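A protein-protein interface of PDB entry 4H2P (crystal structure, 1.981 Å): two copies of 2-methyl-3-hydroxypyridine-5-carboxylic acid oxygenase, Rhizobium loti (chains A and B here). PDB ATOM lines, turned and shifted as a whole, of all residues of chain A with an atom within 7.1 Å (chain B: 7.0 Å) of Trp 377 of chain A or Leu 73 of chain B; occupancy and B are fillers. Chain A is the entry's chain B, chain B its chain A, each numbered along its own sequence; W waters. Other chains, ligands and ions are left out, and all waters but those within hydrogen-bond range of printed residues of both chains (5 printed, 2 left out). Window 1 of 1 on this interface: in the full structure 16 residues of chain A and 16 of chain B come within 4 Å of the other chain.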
ATOM      1  N   HIS A  57     -10.217 -10.576  21.542  1.00  0.00           N
ATOM      2  CA  HIS A  57     -11.144  -9.627  20.922  1.00  0.00           C
ATOM      3  C   HIS A  57     -12.469  -9.486  21.682  1.00  0.00           C
ATOM      4  O   HIS A  57     -12.915  -8.367  21.977  1.00  0.00           O
ATOM      5  CB  HIS A  57     -11.376 -10.030  19.459  1.00  0.00           C
ATOM      6  CG  HIS A  57     -12.564  -9.375  18.824  1.00  0.00           C
ATOM      7  ND1 HIS A  57     -13.782 -10.014  18.704  1.00  0.00           N
ATOM      8  CD2 HIS A  57     -12.710  -8.164  18.227  1.00  0.00           C
ATOM      9  CE1 HIS A  57     -14.636  -9.212  18.089  1.00  0.00           C
ATOM     10  NE2 HIS A  57     -14.012  -8.085  17.792  1.00  0.00           N
ATOM     11  N   ARG A  61     -13.500  -6.088  23.568  1.00  0.00           N
ATOM     12  CA  ARG A  61     -14.679  -5.356  23.133  1.00  0.00           C
ATOM     13  C   ARG A  61     -15.562  -5.048  24.342  1.00  0.00           C
ATOM     14  O   ARG A  61     -16.108  -3.941  24.447  1.00  0.00           O
ATOM     15  CB  ARG A  61     -15.444  -6.135  22.060  1.00  0.00           C
ATOM     16  CG  ARG A  61     -14.768  -6.119  20.685  1.00  0.00           C
ATOM     17  CD  ARG A  61     -14.754  -4.711  20.040  1.00  0.00           C
ATOM     18  NE  ARG A  61     -16.009  -4.450  19.349  1.00  0.00           N
ATOM     19  CZ  ARG A  61     -16.255  -3.385  18.584  1.00  0.00           C
ATOM     20  NH1 ARG A  61     -15.328  -2.459  18.397  1.00  0.00           N
ATOM     21  NH2 ARG A  61     -17.448  -3.249  18.008  1.00  0.00           N
ATOM     22  N   PHE A  96      -3.342 -15.830  14.691  1.00  0.00           N
ATOM     23  CA  PHE A  96      -4.808 -15.745  14.709  1.00  0.00           C
ATOM     24  C   PHE A  96      -5.400 -14.828  13.639  1.00  0.00           C
ATOM     25  O   PHE A  96      -6.462 -14.245  13.848  1.00  0.00           O
ATOM     26  CB  PHE A  96      -5.322 -15.329  16.094  1.00  0.00           C
ATOM     27  CG  PHE A  96      -4.618 -16.016  17.244  1.00  0.00           C
ATOM     28  CD1 PHE A  96      -4.634 -17.391  17.356  1.00  0.00           C
ATOM     29  CD2 PHE A  96      -3.958 -15.278  18.215  1.00  0.00           C
ATOM     30  CE1 PHE A  96      -3.985 -18.023  18.407  1.00  0.00           C
ATOM     31  CE2 PHE A  96      -3.317 -15.900  19.270  1.00  0.00           C
ATOM     32  CZ  PHE A  96      -3.331 -17.275  19.366  1.00  0.00           C
ATOM     33  N   ASN A  97      -4.723 -14.713  12.496  1.00  0.00           N
ATOM     34  CA  ASN A  97      -5.227 -13.894  11.396  1.00  0.00           C
ATOM     35  C   ASN A  97      -5.661 -12.504  11.853  1.00  0.00           C
ATOM     36  O   ASN A  97      -6.723 -12.027  11.466  1.00  0.00           O
ATOM     37  CB  ASN A  97      -6.389 -14.603  10.700  1.00  0.00           C
ATOM     38  CG  ASN A  97      -5.964 -15.924  10.076  1.00  0.00           C
ATOM     39  OD1 ASN A  97      -5.274 -15.937   9.055  1.00  0.00           O
ATOM     40  ND2 ASN A  97      -6.357 -17.042  10.696  1.00  0.00           N
ATOM     41  N   GLY A  98      -4.846 -11.879  12.698  1.00  0.00           N
ATOM     42  CA  GLY A  98      -5.069 -10.501  13.107  1.00  0.00           C
ATOM     43  C   GLY A  98      -6.037 -10.284  14.261  1.00  0.00           C
ATOM     44  O   GLY A  98      -6.197  -9.161  14.734  1.00  0.00           O
ATOM     45  N   LEU A  99      -6.674 -11.353  14.727  1.00  0.00           N
ATOM     46  CA  LEU A  99      -7.602 -11.262  15.852  1.00  0.00           C
ATOM     47  C   LEU A  99      -6.906 -10.676  17.074  1.00  0.00           C
ATOM     48  O   LEU A  99      -5.889 -11.198  17.513  1.00  0.00           O
ATOM     49  CB  LEU A  99      -8.183 -12.641  16.187  1.00  0.00           C
ATOM     50  CG  LEU A  99      -9.370 -12.643  17.169  1.00  0.00           C
ATOM     51  CD1 LEU A  99     -10.429 -13.632  16.750  1.00  0.00           C
ATOM     52  CD2 LEU A  99      -8.896 -12.979  18.555  1.00  0.00           C
ATOM     53  N   PRO A 100      -7.444  -9.577  17.618  1.00  0.00           N
ATOM     54  CA  PRO A 100      -6.788  -8.905  18.742  1.00  0.00           C
ATOM     55  C   PRO A 100      -6.782  -9.758  20.013  1.00  0.00           C
ATOM     56  O   PRO A 100      -7.733 -10.489  20.279  1.00  0.00           O
ATOM     57  CB  PRO A 100      -7.635  -7.644  18.946  1.00  0.00           C
ATOM     58  CG  PRO A 100      -8.286  -7.414  17.633  1.00  0.00           C
ATOM     59  CD  PRO A 100      -8.559  -8.789  17.075  1.00  0.00           C
ATOM     60  N   LEU A 363     -11.657 -20.548  18.202  1.00  0.00           N
ATOM     61  CA  LEU A 363     -11.660 -19.099  18.337  1.00  0.00           C
ATOM     62  C   LEU A 363     -13.060 -18.495  18.228  1.00  0.00           C
ATOM     63  O   LEU A 363     -13.206 -17.283  18.187  1.00  0.00           O
ATOM     64  CB  LEU A 363     -10.724 -18.458  17.300  1.00  0.00           C
ATOM     65  CG  LEU A 363      -9.215 -18.714  17.490  1.00  0.00           C
ATOM     66  CD1 LEU A 363      -8.441 -18.171  16.298  1.00  0.00           C
ATOM     67  CD2 LEU A 363      -8.715 -18.070  18.781  1.00  0.00           C
ATOM     68  N   ALA A 366     -13.816 -15.982  21.065  1.00  0.00           N
ATOM     69  CA  ALA A 366     -12.957 -14.821  20.867  1.00  0.00           C
ATOM     70  C   ALA A 366     -13.417 -13.903  19.711  1.00  0.00           C
ATOM     71  O   ALA A 366     -13.240 -12.688  19.788  1.00  0.00           O
ATOM     72  CB  ALA A 366     -11.510 -15.269  20.655  1.00  0.00           C
ATOM     73  N   ARG A 367     -14.009 -14.481  18.661  1.00  0.00           N
ATOM     74  CA  ARG A 367     -14.419 -13.715  17.470  1.00  0.00           C
ATOM     75  C   ARG A 367     -15.701 -12.942  17.711  1.00  0.00           C
ATOM     76  O   ARG A 367     -16.023 -12.022  16.961  1.00  0.00           O
ATOM     77  CB  ARG A 367     -14.650 -14.621  16.248  1.00  0.00           C
ATOM     78  CG  ARG A 367     -13.442 -15.416  15.765  1.00  0.00           C
ATOM     79  CD  ARG A 367     -13.826 -16.287  14.570  1.00  0.00           C
ATOM     80  NE  ARG A 367     -14.511 -15.461  13.583  1.00  0.00           N
ATOM     81  CZ  ARG A 367     -15.624 -15.803  12.951  1.00  0.00           C
ATOM     82  NH1 ARG A 367     -16.182 -16.988  13.169  1.00  0.00           N
ATOM     83  NH2 ARG A 367     -16.166 -14.953  12.082  1.00  0.00           N
ATOM     84  N   ARG A 372     -21.609  -5.194  18.823  1.00  0.00           N
ATOM     85  CA  ARG A 372     -22.382  -5.203  17.596  1.00  0.00           C
ATOM     86  C   ARG A 372     -23.161  -6.511  17.448  1.00  0.00           C
ATOM     87  O   ARG A 372     -23.961  -6.654  16.542  1.00  0.00           O
ATOM     88  CB  ARG A 372     -21.450  -4.995  16.391  1.00  0.00           C
ATOM     89  CG  ARG A 372     -20.875  -3.595  16.288  1.00  0.00           C
ATOM     90  CD  ARG A 372     -19.500  -3.568  15.622  1.00  0.00           C
ATOM     91  NE  ARG A 372     -19.484  -4.090  14.263  1.00  0.00           N
ATOM     92  CZ  ARG A 372     -18.685  -5.067  13.836  1.00  0.00           C
ATOM     93  NH1 ARG A 372     -17.824  -5.673  14.662  1.00  0.00           N
ATOM     94  NH2 ARG A 372     -18.763  -5.443  12.566  1.00  0.00           N
ATOM     95  N   TYR A 375     -20.054 -11.926  14.730  1.00  0.00           N
ATOM     96  CA  TYR A 375     -18.726 -12.528  14.778  1.00  0.00           C
ATOM     97  C   TYR A 375     -17.795 -11.777  13.829  1.00  0.00           C
ATOM     98  O   TYR A 375     -18.142 -11.531  12.679  1.00  0.00           O
ATOM     99  CB  TYR A 375     -18.779 -14.003  14.404  1.00  0.00           C
ATOM    100  CG  TYR A 375     -19.518 -14.845  15.425  1.00  0.00           C
ATOM    101  CD1 TYR A 375     -20.874 -15.110  15.288  1.00  0.00           C
ATOM    102  CD2 TYR A 375     -18.854 -15.365  16.528  1.00  0.00           C
ATOM    103  CE1 TYR A 375     -21.550 -15.880  16.218  1.00  0.00           C
ATOM    104  CE2 TYR A 375     -19.521 -16.145  17.460  1.00  0.00           C
ATOM    105  CZ  TYR A 375     -20.865 -16.395  17.302  1.00  0.00           C
ATOM    106  OH  TYR A 375     -21.522 -17.160  18.232  1.00  0.00           O
ATOM    107  N   SER A 376     -16.623 -11.400  14.324  1.00  0.00           N
ATOM    108  CA  SER A 376     -15.677 -10.639  13.509  1.00  0.00           C
ATOM    109  C   SER A 376     -14.407 -11.478  13.281  1.00  0.00           C
ATOM    110  O   SER A 376     -14.432 -12.690  13.503  1.00  0.00           O
ATOM    111  CB  SER A 376     -15.373  -9.305  14.206  1.00  0.00           C
ATOM    112  OG  SER A 376     -14.632  -8.425  13.375  1.00  0.00           O
ATOM    113  N   TRP A 377     -13.320 -10.837  12.847  1.00  0.00           N
ATOM    114  CA  TRP A 377     -12.010 -11.484  12.636  1.00  0.00           C
ATOM    115  C   TRP A 377     -12.067 -12.958  12.180  1.00  0.00           C
ATOM    116  O   TRP A 377     -11.675 -13.860  12.919  1.00  0.00           O
ATOM    117  CB  TRP A 377     -11.111 -11.305  13.873  1.00  0.00           C
ATOM    118  CG  TRP A 377     -10.904  -9.841  14.183  1.00  0.00           C
ATOM    119  CD1 TRP A 377     -11.604  -9.078  15.070  1.00  0.00           C
ATOM    120  CD2 TRP A 377      -9.976  -8.962  13.538  1.00  0.00           C
ATOM    121  NE1 TRP A 377     -11.154  -7.776  15.035  1.00  0.00           N
ATOM    122  CE2 TRP A 377     -10.158  -7.678  14.099  1.00  0.00           C
ATOM    123  CE3 TRP A 377      -9.002  -9.139  12.541  1.00  0.00           C
ATOM    124  CZ2 TRP A 377      -9.397  -6.581  13.712  1.00  0.00           C
ATOM    125  CZ3 TRP A 377      -8.250  -8.045  12.149  1.00  0.00           C
ATOM    126  CH2 TRP A 377      -8.449  -6.783  12.736  1.00  0.00           C
ATOM    127  N   PRO A 378     -12.570 -13.189  10.963  1.00  0.00           N
ATOM    128  CA  PRO A 378     -12.798 -14.518  10.392  1.00  0.00           C
ATOM    129  C   PRO A 378     -11.511 -15.333  10.276  1.00  0.00           C
ATOM    130  O   PRO A 378     -10.434 -14.784  10.054  1.00  0.00           O
ATOM    131  CB  PRO A 378     -13.378 -14.206   9.005  1.00  0.00           C
ATOM    132  CG  PRO A 378     -12.900 -12.838   8.694  1.00  0.00           C
ATOM    133  CD  PRO A 378     -12.906 -12.123  10.004  1.00  0.00           C
ATOM    134  N   GLN A 379     -11.626 -16.644  10.440  1.00  0.00           N
ATOM    135  CA  GLN A 379     -10.464 -17.520  10.513  1.00  0.00           C
ATOM    136  C   GLN A 379     -10.453 -18.513   9.355  1.00  0.00           C
ATOM    137  O   GLN A 379      -9.452 -19.175   9.080  1.00  0.00           O
ATOM    138  CB  GLN A 379     -10.474 -18.270  11.844  1.00  0.00           C
ATOM    139  CG  GLN A 379     -10.434 -17.333  13.021  1.00  0.00           C
ATOM    140  CD  GLN A 379      -9.088 -16.653  13.158  1.00  0.00           C
ATOM    141  OE1 GLN A 379      -8.041 -17.283  12.989  1.00  0.00           O
ATOM    142  NE2 GLN A 379      -9.104 -15.361  13.462  1.00  0.00           N
ATOM    143  OXT GLN A 379     -11.458 -18.678   8.671  1.00  0.00           O
ATOM    144  N   LEU B  60      -9.659   0.718   9.931  1.00  0.00           N
ATOM    145  CA  LEU B  60     -10.543  -0.379  10.301  1.00  0.00           C
ATOM    146  C   LEU B  60     -11.681   0.139  11.180  1.00  0.00           C
ATOM    147  O   LEU B  60     -12.815  -0.344  11.098  1.00  0.00           O
ATOM    148  CB  LEU B  60      -9.771  -1.477  11.043  1.00  0.00           C
ATOM    149  CG  LEU B  60      -8.673  -2.150  10.189  1.00  0.00           C
ATOM    150  CD1 LEU B  60      -7.846  -3.119  11.025  1.00  0.00           C
ATOM    151  CD2 LEU B  60      -9.307  -2.879   9.016  1.00  0.00           C
ATOM    152  N   LEU B  63     -14.177   1.738   8.953  1.00  0.00           N
ATOM    153  CA  LEU B  63     -15.002   0.687   8.365  1.00  0.00           C
ATOM    154  C   LEU B  63     -16.064   0.184   9.343  1.00  0.00           C
ATOM    155  O   LEU B  63     -17.189  -0.097   8.946  1.00  0.00           O
ATOM    156  CB  LEU B  63     -14.150  -0.491   7.901  1.00  0.00           C
ATOM    157  CG  LEU B  63     -13.259  -0.174   6.694  1.00  0.00           C
ATOM    158  CD1 LEU B  63     -12.320  -1.317   6.457  1.00  0.00           C
ATOM    159  CD2 LEU B  63     -14.144   0.067   5.487  1.00  0.00           C
ATOM    160  N   ALA B  68     -19.078  -1.642   7.384  1.00  0.00           N
ATOM    161  CA  ALA B  68     -18.449  -2.403   6.317  1.00  0.00           C
ATOM    162  C   ALA B  68     -17.190  -3.167   6.777  1.00  0.00           C
ATOM    163  O   ALA B  68     -16.450  -3.717   5.956  1.00  0.00           O
ATOM    164  CB  ALA B  68     -18.108  -1.475   5.151  1.00  0.00           C
ATOM    165  N   LEU B  69     -16.952  -3.214   8.086  1.00  0.00           N
ATOM    166  CA  LEU B  69     -15.746  -3.863   8.604  1.00  0.00           C
ATOM    167  C   LEU B  69     -15.685  -5.361   8.283  1.00  0.00           C
ATOM    168  O   LEU B  69     -14.682  -5.895   7.786  1.00  0.00           O
ATOM    169  CB  LEU B  69     -15.629  -3.661  10.118  1.00  0.00           C
ATOM    170  CG  LEU B  69     -14.445  -4.380  10.777  1.00  0.00           C
ATOM    171  CD1 LEU B  69     -13.105  -3.827  10.278  1.00  0.00           C
ATOM    172  CD2 LEU B  69     -14.516  -4.287  12.293  1.00  0.00           C
ATOM    173  N   ASP B  70     -16.761  -6.060   8.574  1.00  0.00           N
ATOM    174  CA  ASP B  70     -16.694  -7.503   8.460  1.00  0.00           C
ATOM    175  C   ASP B  70     -16.668  -7.975   7.009  1.00  0.00           C
ATOM    176  O   ASP B  70     -16.082  -9.006   6.713  1.00  0.00           O
ATOM    177  CB  ASP B  70     -17.778  -8.156   9.311  1.00  0.00           C
ATOM    178  CG  ASP B  70     -17.560  -7.892  10.806  1.00  0.00           C
ATOM    179  OD1 ASP B  70     -16.395  -8.006  11.283  1.00  0.00           O
ATOM    180  OD2 ASP B  70     -18.539  -7.541  11.497  1.00  0.00           O
ATOM    181  N   ASP B  71     -17.245  -7.192   6.100  1.00  0.00           N
ATOM    182  CA  ASP B  71     -17.150  -7.496   4.667  1.00  0.00           C
ATOM    183  C   ASP B  71     -15.714  -7.336   4.156  1.00  0.00           C
ATOM    184  O   ASP B  71     -15.293  -8.026   3.226  1.00  0.00           O
ATOM    185  CB  ASP B  71     -18.059  -6.591   3.844  1.00  0.00           C
ATOM    186  CG  ASP B  71     -19.535  -6.809   4.147  1.00  0.00           C
ATOM    187  OD1 ASP B  71     -19.964  -7.983   4.248  1.00  0.00           O
ATOM    188  OD2 ASP B  71     -20.258  -5.799   4.293  1.00  0.00           O
ATOM    189  N   VAL B  72     -14.982  -6.406   4.758  1.00  0.00           N
ATOM    190  CA  VAL B  72     -13.574  -6.207   4.417  1.00  0.00           C
ATOM    191  C   VAL B  72     -12.686  -7.287   5.059  1.00  0.00           C
ATOM    192  O   VAL B  72     -11.812  -7.861   4.397  1.00  0.00           O
ATOM    193  CB  VAL B  72     -13.091  -4.783   4.823  1.00  0.00           C
ATOM    194  CG1 VAL B  72     -11.576  -4.681   4.770  1.00  0.00           C
ATOM    195  CG2 VAL B  72     -13.739  -3.709   3.913  1.00  0.00           C
ATOM    196  N   LEU B  73     -12.907  -7.585   6.339  1.00  0.00           N
ATOM    197  CA  LEU B  73     -12.065  -8.579   7.010  1.00  0.00           C
ATOM    198  C   LEU B  73     -12.146  -9.957   6.349  1.00  0.00           C
ATOM    199  O   LEU B  73     -11.149 -10.673   6.252  1.00  0.00           O
ATOM    200  CB  LEU B  73     -12.383  -8.677   8.503  1.00  0.00           C
ATOM    201  CG  LEU B  73     -12.031  -7.447   9.357  1.00  0.00           C
ATOM    202  CD1 LEU B  73     -12.329  -7.717  10.835  1.00  0.00           C
ATOM    203  CD2 LEU B  73     -10.558  -7.041   9.185  1.00  0.00           C
ATOM    204  N   GLN B  74     -13.335 -10.331   5.893  1.00  0.00           N
ATOM    205  CA  GLN B  74     -13.492 -11.588   5.189  1.00  0.00           C
ATOM    206  C   GLN B  74     -12.836 -11.457   3.813  1.00  0.00           C
ATOM    207  O   GLN B  74     -13.297 -10.678   2.994  1.00  0.00           O
ATOM    208  CB  GLN B  74     -14.981 -11.923   5.048  1.00  0.00           C
ATOM    209  CG  GLN B  74     -15.269 -13.232   4.342  1.00  0.00           C
ATOM    210  CD  GLN B  74     -14.795 -14.434   5.138  1.00  0.00           C
ATOM    211  OE1 GLN B  74     -15.283 -14.698   6.236  1.00  0.00           O
ATOM    212  NE2 GLN B  74     -13.825 -15.160   4.592  1.00  0.00           N
ATOM    213  N   GLY B  75     -11.759 -12.208   3.563  1.00  0.00           N
ATOM    214  CA  GLY B  75     -11.058 -12.124   2.295  1.00  0.00           C
ATOM    215  C   GLY B  75      -9.882 -11.151   2.261  1.00  0.00           C
ATOM    216  O   GLY B  75      -9.367 -10.822   1.184  1.00  0.00           O
ATOM    217  N   SER B  76      -9.457 -10.671   3.424  1.00  0.00           N
ATOM    218  CA  SER B  76      -8.202  -9.907   3.544  1.00  0.00           C
ATOM    219  C   SER B  76      -7.273 -10.591   4.556  1.00  0.00           C
ATOM    220  O   SER B  76      -7.611 -11.655   5.064  1.00  0.00           O
ATOM    221  CB  SER B  76      -8.476  -8.446   3.921  1.00  0.00           C
ATOM    222  OG  SER B  76      -9.254  -8.365   5.114  1.00  0.00           O
ATOM    223  N   HIS B  77      -6.120  -9.991   4.860  1.00  0.00           N
ATOM    224  CA  HIS B  77      -5.043 -10.725   5.531  1.00  0.00           C
ATOM    225  C   HIS B  77      -4.289  -9.849   6.532  1.00  0.00           C
ATOM    226  O   HIS B  77      -3.959  -8.705   6.230  1.00  0.00           O
ATOM    227  CB  HIS B  77      -4.078 -11.263   4.444  1.00  0.00           C
ATOM    228  CG  HIS B  77      -2.834 -11.931   4.968  1.00  0.00           C
ATOM    229  ND1 HIS B  77      -2.848 -13.176   5.567  1.00  0.00           N
ATOM    230  CD2 HIS B  77      -1.528 -11.565   4.897  1.00  0.00           C
ATOM    231  CE1 HIS B  77      -1.611 -13.522   5.888  1.00  0.00           C
ATOM    232  NE2 HIS B  77      -0.792 -12.564   5.490  1.00  0.00           N
ATOM    233  N   THR B  78      -4.021 -10.369   7.725  1.00  0.00           N
ATOM    234  CA  THR B  78      -3.028  -9.740   8.600  1.00  0.00           C
ATOM    235  C   THR B  78      -1.790 -10.623   8.715  1.00  0.00           C
ATOM    236  O   THR B  78      -1.856 -11.703   9.304  1.00  0.00           O
ATOM    237  CB  THR B  78      -3.528  -9.539  10.052  1.00  0.00           C
ATOM    238  OG1 THR B  78      -4.737  -8.779  10.069  1.00  0.00           O
ATOM    239  CG2 THR B  78      -2.450  -8.827  10.876  1.00  0.00           C
ATOM    240  N   PRO B 100      -4.132  -3.388  15.483  1.00  0.00           N
ATOM    241  CA  PRO B 100      -4.741  -4.062  14.332  1.00  0.00           C
ATOM    242  C   PRO B 100      -4.327  -3.469  12.979  1.00  0.00           C
ATOM    243  O   PRO B 100      -4.216  -2.254  12.837  1.00  0.00           O
ATOM    244  CB  PRO B 100      -6.244  -3.871  14.568  1.00  0.00           C
ATOM    245  CG  PRO B 100      -6.368  -3.657  16.043  1.00  0.00           C
ATOM    246  CD  PRO B 100      -5.145  -2.871  16.418  1.00  0.00           C
ATOM    247  N   TRP B 101      -4.077  -4.335  12.000  1.00  0.00           N
ATOM    248  CA  TRP B 101      -3.745  -3.902  10.645  1.00  0.00           C
ATOM    249  C   TRP B 101      -4.153  -5.002   9.652  1.00  0.00           C
ATOM    250  O   TRP B 101      -4.500  -6.119  10.057  1.00  0.00           O
ATOM    251  CB  TRP B 101      -2.263  -3.499  10.520  1.00  0.00           C
ATOM    252  CG  TRP B 101      -1.274  -4.599  10.774  1.00  0.00           C
ATOM    253  CD1 TRP B 101      -1.086  -5.270  11.938  1.00  0.00           C
ATOM    254  CD2 TRP B 101      -0.311  -5.119   9.844  1.00  0.00           C
ATOM    255  NE1 TRP B 101      -0.076  -6.196  11.793  1.00  0.00           N
ATOM    256  CE2 TRP B 101       0.414  -6.123  10.515  1.00  0.00           C
ATOM    257  CE3 TRP B 101       0.000  -4.838   8.506  1.00  0.00           C
ATOM    258  CZ2 TRP B 101       1.431  -6.851   9.900  1.00  0.00           C
ATOM    259  CZ3 TRP B 101       1.026  -5.565   7.894  1.00  0.00           C
ATOM    260  CH2 TRP B 101       1.726  -6.549   8.595  1.00  0.00           C
ATOM    261  N   ARG B 102      -4.164  -4.685   8.362  1.00  0.00           N
ATOM    262  CA  ARG B 102      -4.794  -5.562   7.384  1.00  0.00           C
ATOM    263  C   ARG B 102      -4.296  -5.189   5.996  1.00  0.00           C
ATOM    264  O   ARG B 102      -4.119  -4.015   5.699  1.00  0.00           O
ATOM    265  CB  ARG B 102      -6.317  -5.383   7.422  1.00  0.00           C
ATOM    266  CG  ARG B 102      -7.116  -6.560   6.866  1.00  0.00           C
ATOM    267  CD  ARG B 102      -6.939  -7.770   7.807  1.00  0.00           C
ATOM    268  NE  ARG B 102      -7.903  -8.843   7.583  1.00  0.00           N
ATOM    269  CZ  ARG B 102      -8.004  -9.909   8.375  1.00  0.00           C
ATOM    270  NH1 ARG B 102      -7.194 -10.041   9.424  1.00  0.00           N
ATOM    271  NH2 ARG B 102      -8.917 -10.839   8.123  1.00  0.00           N
ATOM    272  N   MET B 104      -5.084  -5.887   1.774  1.00  0.00           N
ATOM    273  CA  MET B 104      -6.169  -6.351   0.915  1.00  0.00           C
ATOM    274  C   MET B 104      -5.972  -5.808  -0.492  1.00  0.00           C
ATOM    275  O   MET B 104      -5.241  -4.841  -0.675  1.00  0.00           O
ATOM    276  CB  MET B 104      -7.498  -5.831   1.475  1.00  0.00           C
ATOM    277  CG  MET B 104      -7.579  -4.315   1.497  1.00  0.00           C
ATOM    278  SD  MET B 104      -8.729  -3.710   2.740  1.00  0.00           S
ATOM    279  CE  MET B 104      -7.719  -4.022   4.212  1.00  0.00           C
ATOM    280  N   HIS B 108     -11.016  -5.247  -3.385  1.00  0.00           N
ATOM    281  CA  HIS B 108     -11.715  -5.839  -2.244  1.00  0.00           C
ATOM    282  C   HIS B 108     -12.283  -4.728  -1.355  1.00  0.00           C
ATOM    283  O   HIS B 108     -13.465  -4.742  -1.000  1.00  0.00           O
ATOM    284  CB  HIS B 108     -10.776  -6.746  -1.441  1.00  0.00           C
ATOM    285  CG  HIS B 108     -11.463  -7.478  -0.326  1.00  0.00           C
ATOM    286  ND1 HIS B 108     -12.402  -8.465  -0.552  1.00  0.00           N
ATOM    287  CD2 HIS B 108     -11.350  -7.367   1.022  1.00  0.00           C
ATOM    288  CE1 HIS B 108     -12.830  -8.935   0.608  1.00  0.00           C
ATOM    289  NE2 HIS B 108     -12.209  -8.285   1.577  1.00  0.00           N
HETATM  290  O   HOH W   1      -1.880 -12.336  12.031  1.00  0.00           O
HETATM  291  O   HOH W   2      -2.216 -14.602   8.977  1.00  0.00           O
HETATM  292  O   HOH W   3      -4.720  -7.319  13.270  1.00  0.00           O
HETATM  293  O   HOH W   4      -9.329 -12.313  10.573  1.00  0.00           O
HETATM  294  O   HOH W   5      -4.930 -13.103   8.227  1.00  0.00           O
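The backbone carbonyl oxygen (O) of Leu 73 of chain B lies within hydrogen-bond range of the side-chain hydroxyl (OG) of Ser 76 of chain B, 3.2 Å away.
The backbone carbonyl oxygen of Leu 73 of chain B lies within hydrogen-bond range of the guanidinium group of Arg 102 of chain B, at 2.9 Å.
OE1 of Gln 379 of chain A lies within hydrogen-bond range of ND2 of Asn 97 of chain A (2.9 Å).
The guanidinium group (NE) of Arg 367 of chain A sits at hydrogen-bond distance from the backbone carbonyl oxygen (O) of Ser 376 of chain A, at 2.8 Å.
The backbone carbonyl oxygen of Trp 377 of chain A lies within hydrogen-bond range of the guanidinium group of Arg 367 of chain A (3.3 Å).
The backbone carbonyl oxygen of Trp 377 of chain A lies within hydrogen-bond range of the side-chain amide nitrogen of Gln 379 of chain A (3.0 Å).
1 position is printed for both chains.
Of the 9 pairs that touch across the chains among the printed residues, none has its exchanged pair printed and touching as well.
CA of Gly 98 of chain A touches OG1 of Thr 78 of chain B, 3.5 Å away.
Leu 73 of chain B touches Ser 376 of chain A (CD1 to OG, 3.5 Å).
CD2 of Trp 377 of chain A touches CD1 of Leu 73 of chain B (3.8 Å).
Trp 377 of chain A touches Arg 102 of chain B.
Pro 378 of chain A touches Leu 73 of chain B.
Pro 378 of chain A touches Gln 74 of chain B (CB to OE1, 3.4 Å).
OD1 of Asp 70 of chain B is in salt-bridge range of NH2 of Arg 372 of chain A, at 3.7 Å.
The side-chain hydroxyl of Ser 376 of chain A lies within hydrogen-bond range of the side-chain carboxylate of Asp 70 of chain B (2.8 Å).
The guanidinium group (NH1) of Arg 102 of chain B sits at hydrogen-bond distance from the backbone carbonyl oxygen (O) of Asn 97 of chain A.
Water W4 lies within hydrogen-bond range of O of Pro 378 of chain A (2.8 Å), O of Asn 97 of chain A (2.8 Å) and NH2 of Arg 102 of chain B (2.9 Å).
Water W3 lies within hydrogen-bond range of O of Gly 98 of chain A (2.8 Å) and N of Trp 101 of chain B (3.3 Å).
Water W1 lies within hydrogen-bond range of the backbone carbonyl oxygen of Thr 78 of chain B (2.8 Å) and the backbone NH of Gly 98 of chain A (3.1 Å).
Water W5 lies within hydrogen-bond range of N of Thr 78 of chain B, OD1 of Asn 97 of chain A and ND1 of His 77 of chain B.
Water W2 lies within hydrogen-bond range of the backbone carbonyl oxygen of Thr 78 of chain B (2.9 Å) and the side-chain amide oxygen of Asn 97 of chain A (3.3 Å).
Hydrophobic or aromatic side chains of chain A that line the printed part of chain B: Trp 377 and Pro 378.
Of the 18 printed residues of chain B, 5 touch a printed residue of chain A.
Hydrophobic or aromatic side chains of chain B within 4 Å of the printed part of chain A: Leu 73.
Among the printed residues, 9 pairs touch across the chains.
Trp 377 of chain A touches just these residues of chain B: Leu 73 and Arg 102.
Of the printed residues of chain A, Leu 73 of chain B touches Ser 376, Trp 377 and Pro 378.
Printed residues of chain B within 4 Å of Gly 98 of chain A: Thr 78.
Of the printed residues of chain A, Arg 102 of chain B touches Asn 97 (2.9 Å) and Trp 377 (3.5 Å).
Of the printed residues of chain B, Asn 97 of chain A touches Arg 102 (2.9 Å).
Printed residues of chain B within 4 Å of Pro 378 of chain A: Leu 73 and Gln 74.
The nearest printed residue of chain B that does not touch Trp 377 of chain A is Pro 100 of chain B (4.1 Å).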
